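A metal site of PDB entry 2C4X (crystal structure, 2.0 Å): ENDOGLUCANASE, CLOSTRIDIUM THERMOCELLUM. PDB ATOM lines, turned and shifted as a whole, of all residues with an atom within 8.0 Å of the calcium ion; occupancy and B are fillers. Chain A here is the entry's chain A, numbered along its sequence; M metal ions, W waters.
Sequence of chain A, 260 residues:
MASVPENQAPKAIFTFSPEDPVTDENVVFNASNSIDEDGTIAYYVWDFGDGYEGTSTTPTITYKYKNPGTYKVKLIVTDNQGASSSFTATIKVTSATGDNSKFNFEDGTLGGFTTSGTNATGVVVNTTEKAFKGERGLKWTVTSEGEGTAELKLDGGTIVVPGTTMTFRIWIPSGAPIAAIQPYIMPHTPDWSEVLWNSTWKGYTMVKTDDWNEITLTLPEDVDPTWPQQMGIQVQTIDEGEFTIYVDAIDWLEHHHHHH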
ATOM      1  N   GLU A   6     -26.178 -37.954  13.386  1.00  0.00           N
ATOM      2  CA  GLU A   6     -27.152 -37.103  12.670  1.00  0.00           C
ATOM      3  C   GLU A   6     -27.405 -35.720  13.278  1.00  0.00           C
ATOM      4  O   GLU A   6     -27.744 -35.592  14.456  1.00  0.00           O
ATOM      5  CB  GLU A   6     -28.491 -37.850  12.524  1.00  0.00           C
ATOM      6  CG  GLU A   6     -28.703 -38.496  11.167  1.00  0.00           C
ATOM      7  CD  GLU A   6     -29.339 -37.552  10.145  1.00  0.00           C
ATOM      8  OE1 GLU A   6     -30.220 -36.757  10.530  1.00  0.00           O
ATOM      9  OE2 GLU A   6     -28.959 -37.630   8.947  1.00  0.00           O
ATOM     10  N   ASN A   7     -27.278 -34.685  12.438  1.00  0.00           N
ATOM     11  CA  ASN A   7     -27.516 -33.304  12.872  1.00  0.00           C
ATOM     12  C   ASN A   7     -28.961 -33.063  13.348  1.00  0.00           C
ATOM     13  O   ASN A   7     -29.914 -33.377  12.628  1.00  0.00           O
ATOM     14  CB  ASN A   7     -27.173 -32.315  11.745  1.00  0.00           C
ATOM     15  CG  ASN A   7     -27.441 -30.871  12.133  1.00  0.00           C
ATOM     16  OD1 ASN A   7     -27.205 -30.463  13.265  1.00  0.00           O
ATOM     17  ND2 ASN A   7     -27.924 -30.084  11.186  1.00  0.00           N
ATOM     18  N   GLN A   8     -29.108 -32.509  14.553  1.00  0.00           N
ATOM     19  CA  GLN A   8     -30.417 -32.085  15.048  1.00  0.00           C
ATOM     20  C   GLN A   8     -30.777 -30.717  14.474  1.00  0.00           C
ATOM     21  O   GLN A   8     -29.934 -29.797  14.461  1.00  0.00           O
ATOM     22  CB  GLN A   8     -30.434 -32.020  16.578  1.00  0.00           C
ATOM     23  CG  GLN A   8     -30.259 -33.352  17.240  1.00  0.00           C
ATOM     24  CD  GLN A   8     -30.082 -33.238  18.748  1.00  0.00           C
ATOM     25  OE1 GLN A   8     -30.627 -32.345  19.400  1.00  0.00           O
ATOM     26  NE2 GLN A   8     -29.304 -34.143  19.301  1.00  0.00           N
ATOM     27  N   ALA A   9     -32.022 -30.591  14.014  1.00  0.00           N
ATOM     28  CA  ALA A   9     -32.531 -29.309  13.534  1.00  0.00           C
ATOM     29  C   ALA A   9     -32.707 -28.348  14.712  1.00  0.00           C
ATOM     30  O   ALA A   9     -33.047 -28.781  15.812  1.00  0.00           O
ATOM     31  CB  ALA A   9     -33.853 -29.486  12.782  1.00  0.00           C
ATOM     32  N   PRO A  10     -32.439 -27.046  14.502  1.00  0.00           N
ATOM     33  CA  PRO A  10     -32.528 -26.106  15.600  1.00  0.00           C
ATOM     34  C   PRO A  10     -33.987 -25.917  16.043  1.00  0.00           C
ATOM     35  O   PRO A  10     -34.904 -26.348  15.341  1.00  0.00           O
ATOM     36  CB  PRO A  10     -31.968 -24.799  15.019  1.00  0.00           C
ATOM     37  CG  PRO A  10     -32.096 -24.952  13.524  1.00  0.00           C
ATOM     38  CD  PRO A  10     -32.036 -26.425  13.226  1.00  0.00           C
ATOM     39  N   LYS A  11     -34.190 -25.317  17.207  1.00  0.00           N
ATOM     40  CA  LYS A  11     -35.554 -25.014  17.658  1.00  0.00           C
ATOM     41  C   LYS A  11     -35.871 -23.541  17.429  1.00  0.00           C
ATOM     42  O   LYS A  11     -35.102 -22.665  17.825  1.00  0.00           O
ATOM     43  CB  LYS A  11     -35.764 -25.479  19.088  1.00  0.00           C
ATOM     44  CG  LYS A  11     -35.713 -27.027  19.172  1.00  0.00           C
ATOM     45  CD  LYS A  11     -36.245 -27.642  20.468  1.00  0.00           C
ATOM     46  CE  LYS A  11     -37.798 -27.634  20.520  1.00  0.00           C
ATOM     47  NZ  LYS A  11     -38.529 -28.165  19.313  1.00  0.00           N
ATOM     48  N   ILE A  35     -32.741 -22.000  19.577  1.00  0.00           N
ATOM     49  CA  ILE A  35     -31.460 -22.619  19.906  1.00  0.00           C
ATOM     50  C   ILE A  35     -31.159 -23.823  19.023  1.00  0.00           C
ATOM     51  O   ILE A  35     -32.074 -24.555  18.631  1.00  0.00           O
ATOM     52  CB  ILE A  35     -31.394 -22.994  21.431  1.00  0.00           C
ATOM     53  CG1 ILE A  35     -29.998 -23.513  21.813  1.00  0.00           C
ATOM     54  CG2 ILE A  35     -32.524 -23.954  21.818  1.00  0.00           C
ATOM     55  CD1 ILE A  35     -29.739 -23.562  23.339  1.00  0.00           C
ATOM     56  N   ASP A  36     -29.896 -23.992  18.656  1.00  0.00           N
ATOM     57  CA  ASP A  36     -29.439 -25.242  18.090  1.00  0.00           C
ATOM     58  C   ASP A  36     -28.742 -26.015  19.201  1.00  0.00           C
ATOM     59  O   ASP A  36     -27.781 -25.511  19.804  1.00  0.00           O
ATOM     60  CB  ASP A  36     -28.519 -25.037  16.894  1.00  0.00           C
ATOM     61  CG  ASP A  36     -28.324 -26.302  16.106  1.00  0.00           C
ATOM     62  OD1 ASP A  36     -29.302 -27.069  15.985  1.00  0.00           O
ATOM     63  OD2 ASP A  36     -27.212 -26.552  15.608  1.00  0.00           O
ATOM     64  N   GLU A  37     -29.223 -27.219  19.471  1.00  0.00           N
ATOM     65  CA  GLU A  37     -28.723 -28.024  20.573  1.00  0.00           C
ATOM     66  C   GLU A  37     -27.331 -28.617  20.322  1.00  0.00           C
ATOM     67  O   GLU A  37     -26.575 -28.829  21.278  1.00  0.00           O
ATOM     68  CB  GLU A  37     -29.729 -29.124  20.933  1.00  0.00           C
ATOM     69  CG  GLU A  37     -31.167 -28.612  21.131  1.00  0.00           C
ATOM     70  CD  GLU A  37     -31.345 -27.794  22.406  1.00  0.00           C
ATOM     71  OE1 GLU A  37     -30.445 -27.796  23.274  1.00  0.00           O
ATOM     72  OE2 GLU A  37     -32.413 -27.166  22.543  1.00  0.00           O
ATOM     73  N   ASP A  38     -27.001 -28.879  19.057  1.00  0.00           N
ATOM     74  CA  ASP A  38     -25.734 -29.551  18.727  1.00  0.00           C
ATOM     75  C   ASP A  38     -24.846 -28.696  17.803  1.00  0.00           C
ATOM     76  O   ASP A  38     -23.926 -29.214  17.164  1.00  0.00           O
ATOM     77  CB  ASP A  38     -25.994 -30.936  18.119  1.00  0.00           C
ATOM     78  CG  ASP A  38     -26.761 -30.876  16.790  1.00  0.00           C
ATOM     79  OD1 ASP A  38     -27.243 -29.790  16.432  1.00  0.00           O
ATOM     80  OD2 ASP A  38     -26.891 -31.917  16.110  1.00  0.00           O
ATOM     81  N   GLY A  39     -25.122 -27.404  17.743  1.00  0.00           N
ATOM     82  CA  GLY A  39     -24.358 -26.501  16.889  1.00  0.00           C
ATOM     83  C   GLY A  39     -24.714 -25.077  17.231  1.00  0.00           C
ATOM     84  O   GLY A  39     -24.929 -24.753  18.406  1.00  0.00           O
ATOM     85  N   THR A  40     -24.773 -24.225  16.217  1.00  0.00           N
ATOM     86  CA  THR A  40     -25.151 -22.828  16.388  1.00  0.00           C
ATOM     87  C   THR A  40     -26.158 -22.410  15.322  1.00  0.00           C
ATOM     88  O   THR A  40     -26.239 -23.026  14.261  1.00  0.00           O
ATOM     89  CB  THR A  40     -23.916 -21.885  16.328  1.00  0.00           C
ATOM     90  OG1 THR A  40     -23.224 -22.079  15.096  1.00  0.00           O
ATOM     91  CG2 THR A  40     -22.938 -22.171  17.482  1.00  0.00           C
ATOM     92  N   ILE A  41     -26.937 -21.370  15.598  1.00  0.00           N
ATOM     93  CA  ILE A  41     -27.858 -20.832  14.605  1.00  0.00           C
ATOM     94  C   ILE A  41     -27.077 -19.882  13.697  1.00  0.00           C
ATOM     95  O   ILE A  41     -26.385 -18.986  14.195  1.00  0.00           O
ATOM     96  CB  ILE A  41     -29.054 -20.111  15.256  1.00  0.00           C
ATOM     97  CG1 ILE A  41     -29.951 -21.133  15.963  1.00  0.00           C
ATOM     98  CG2 ILE A  41     -29.853 -19.311  14.190  1.00  0.00           C
ATOM     99  CD1 ILE A  41     -30.917 -20.512  16.949  1.00  0.00           C
ATOM    100  N   THR A  78     -32.052 -21.348  10.877  1.00  0.00           N
ATOM    101  CA  THR A  78     -31.185 -22.288  10.190  1.00  0.00           C
ATOM    102  C   THR A  78     -29.872 -22.402  10.952  1.00  0.00           C
ATOM    103  O   THR A  78     -29.286 -21.384  11.335  1.00  0.00           O
ATOM    104  CB  THR A  78     -30.945 -21.841   8.723  1.00  0.00           C
ATOM    105  OG1 THR A  78     -32.206 -21.609   8.098  1.00  0.00           O
ATOM    106  CG2 THR A  78     -30.152 -22.881   7.924  1.00  0.00           C
ATOM    107  N   ASP A  79     -29.435 -23.635  11.170  1.00  0.00           N
ATOM    108  CA  ASP A  79     -28.186 -23.881  11.904  1.00  0.00           C
ATOM    109  C   ASP A  79     -26.946 -23.873  10.997  1.00  0.00           C
ATOM    110  O   ASP A  79     -27.052 -23.677   9.770  1.00  0.00           O
ATOM    111  CB  ASP A  79     -28.288 -25.161  12.762  1.00  0.00           C
ATOM    112  CG  ASP A  79     -28.302 -26.437  11.955  1.00  0.00           C
ATOM    113  OD1 ASP A  79     -27.893 -26.435  10.781  1.00  0.00           O
ATOM    114  OD2 ASP A  79     -28.701 -27.482  12.498  1.00  0.00           O
ATOM    115  N   ASN A  80     -25.770 -24.069  11.609  1.00  0.00           N
ATOM    116  CA  ASN A  80     -24.480 -24.074  10.914  1.00  0.00           C
ATOM    117  C   ASN A  80     -24.297 -25.169   9.851  1.00  0.00           C
ATOM    118  O   ASN A  80     -23.389 -25.106   9.026  1.00  0.00           O
ATOM    119  CB  ASN A  80     -23.333 -24.141  11.944  1.00  0.00           C
ATOM    120  CG  ASN A  80     -23.383 -25.393  12.809  1.00  0.00           C
ATOM    121  OD1 ASN A  80     -24.313 -25.590  13.583  1.00  0.00           O
ATOM    122  ND2 ASN A  80     -22.364 -26.242  12.701  1.00  0.00           N
ATOM    123  N   GLN A  81     -25.176 -26.174   9.887  1.00  0.00           N
ATOM    124  CA  GLN A  81     -25.142 -27.268   8.926  1.00  0.00           C
ATOM    125  C   GLN A  81     -26.291 -27.241   7.910  1.00  0.00           C
ATOM    126  O   GLN A  81     -26.463 -28.173   7.137  1.00  0.00           O
ATOM    127  CB  GLN A  81     -25.108 -28.596   9.679  1.00  0.00           C
ATOM    128  CG  GLN A  81     -23.719 -28.921  10.240  1.00  0.00           C
ATOM    129  CD  GLN A  81     -23.730 -30.114  11.156  1.00  0.00           C
ATOM    130  OE1 GLN A  81     -23.258 -31.193  10.779  1.00  0.00           O
ATOM    131  NE2 GLN A  81     -24.272 -29.958  12.364  1.00  0.00           N
ATOM    132  N   GLY A  82     -27.072 -26.161   7.918  1.00  0.00           N
ATOM    133  CA  GLY A  82     -28.155 -25.972   6.955  1.00  0.00           C
ATOM    134  C   GLY A  82     -29.509 -26.596   7.260  1.00  0.00           C
ATOM    135  O   GLY A  82     -30.412 -26.554   6.420  1.00  0.00           O
ATOM    136  N   ALA A  83     -29.662 -27.170   8.454  1.00  0.00           N
ATOM    137  CA  ALA A  83     -30.978 -27.671   8.896  1.00  0.00           C
ATOM    138  C   ALA A  83     -31.798 -26.533   9.495  1.00  0.00           C
ATOM    139  O   ALA A  83     -31.260 -25.602  10.110  1.00  0.00           O
ATOM    140  CB  ALA A  83     -30.819 -28.820   9.911  1.00  0.00           C
ATOM    141  N   SER A  84     -33.111 -26.606   9.309  1.00  0.00           N
ATOM    142  CA  SER A  84     -33.975 -25.524   9.758  1.00  0.00           C
ATOM    143  C   SER A  84     -35.273 -25.996  10.412  1.00  0.00           C
ATOM    144  O   SER A  84     -35.705 -27.128  10.212  1.00  0.00           O
ATOM    145  CB  SER A  84     -34.254 -24.565   8.602  1.00  0.00           C
ATOM    146  OG  SER A  84     -34.891 -25.239   7.548  1.00  0.00           O
HETATM  147 CA    CA M   1     -27.888 -28.539  14.538  1.00  0.00          CA
HETATM  148  O   HOH W   1     -25.689 -28.000  13.709  1.00  0.00           O
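OD2 of Asp 36 is bound to the calcium ion, 2.4 Å away.
The calcium ion is bound by OD1 of Asp 38.
The backbone carbonyl oxygen (O) of Gln 8 is bound to the calcium ion (2.4 Å).
The side-chain amide oxygen (OD1) of Asn 7 is bound to the calcium ion.
Water W1 is bound to the calcium ion, 2.4 Å away.
The side-chain carboxylate (OD2) of Asp 79 is bound to the calcium ion.
OD1 of Asp 36 binds the calcium ion (2.5 Å).
Water W1 lies within hydrogen-bond range of NE2 of Gln 81 (2.8 Å) and OD1 of Asn 80 (2.8 Å).
Within 4 Å of the calcium ion: Asn 7, Gln 8, Asp 36, Asp 38 and Asp 79.
The nearest printed residue that does not touch the calcium ion is Gly 39 (4.4 Å).
The side-chain carboxylate (OD2) of Asp 36 lies close to the backbone NH (N) of Gly 39 (3.1 Å).
The side-chain carboxylate of Asp 36 sits close to the backbone NH of Thr 40 (3.4 Å).
OD1 of Asn 7 lies close to NE2 of Gln 81.
The backbone NH of Gln 81 sits at hydrogen-bond distance from the side-chain carboxylate of Asp 79, at 2.9 Å.
The side-chain carboxylate (OD1) of Asp 79 sits at hydrogen-bond distance from the backbone NH (N) of Ala 83 (3.0 Å).
The side-chain carboxylate of Asp 79 lies within hydrogen-bond range of the backbone NH of Gly 82.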
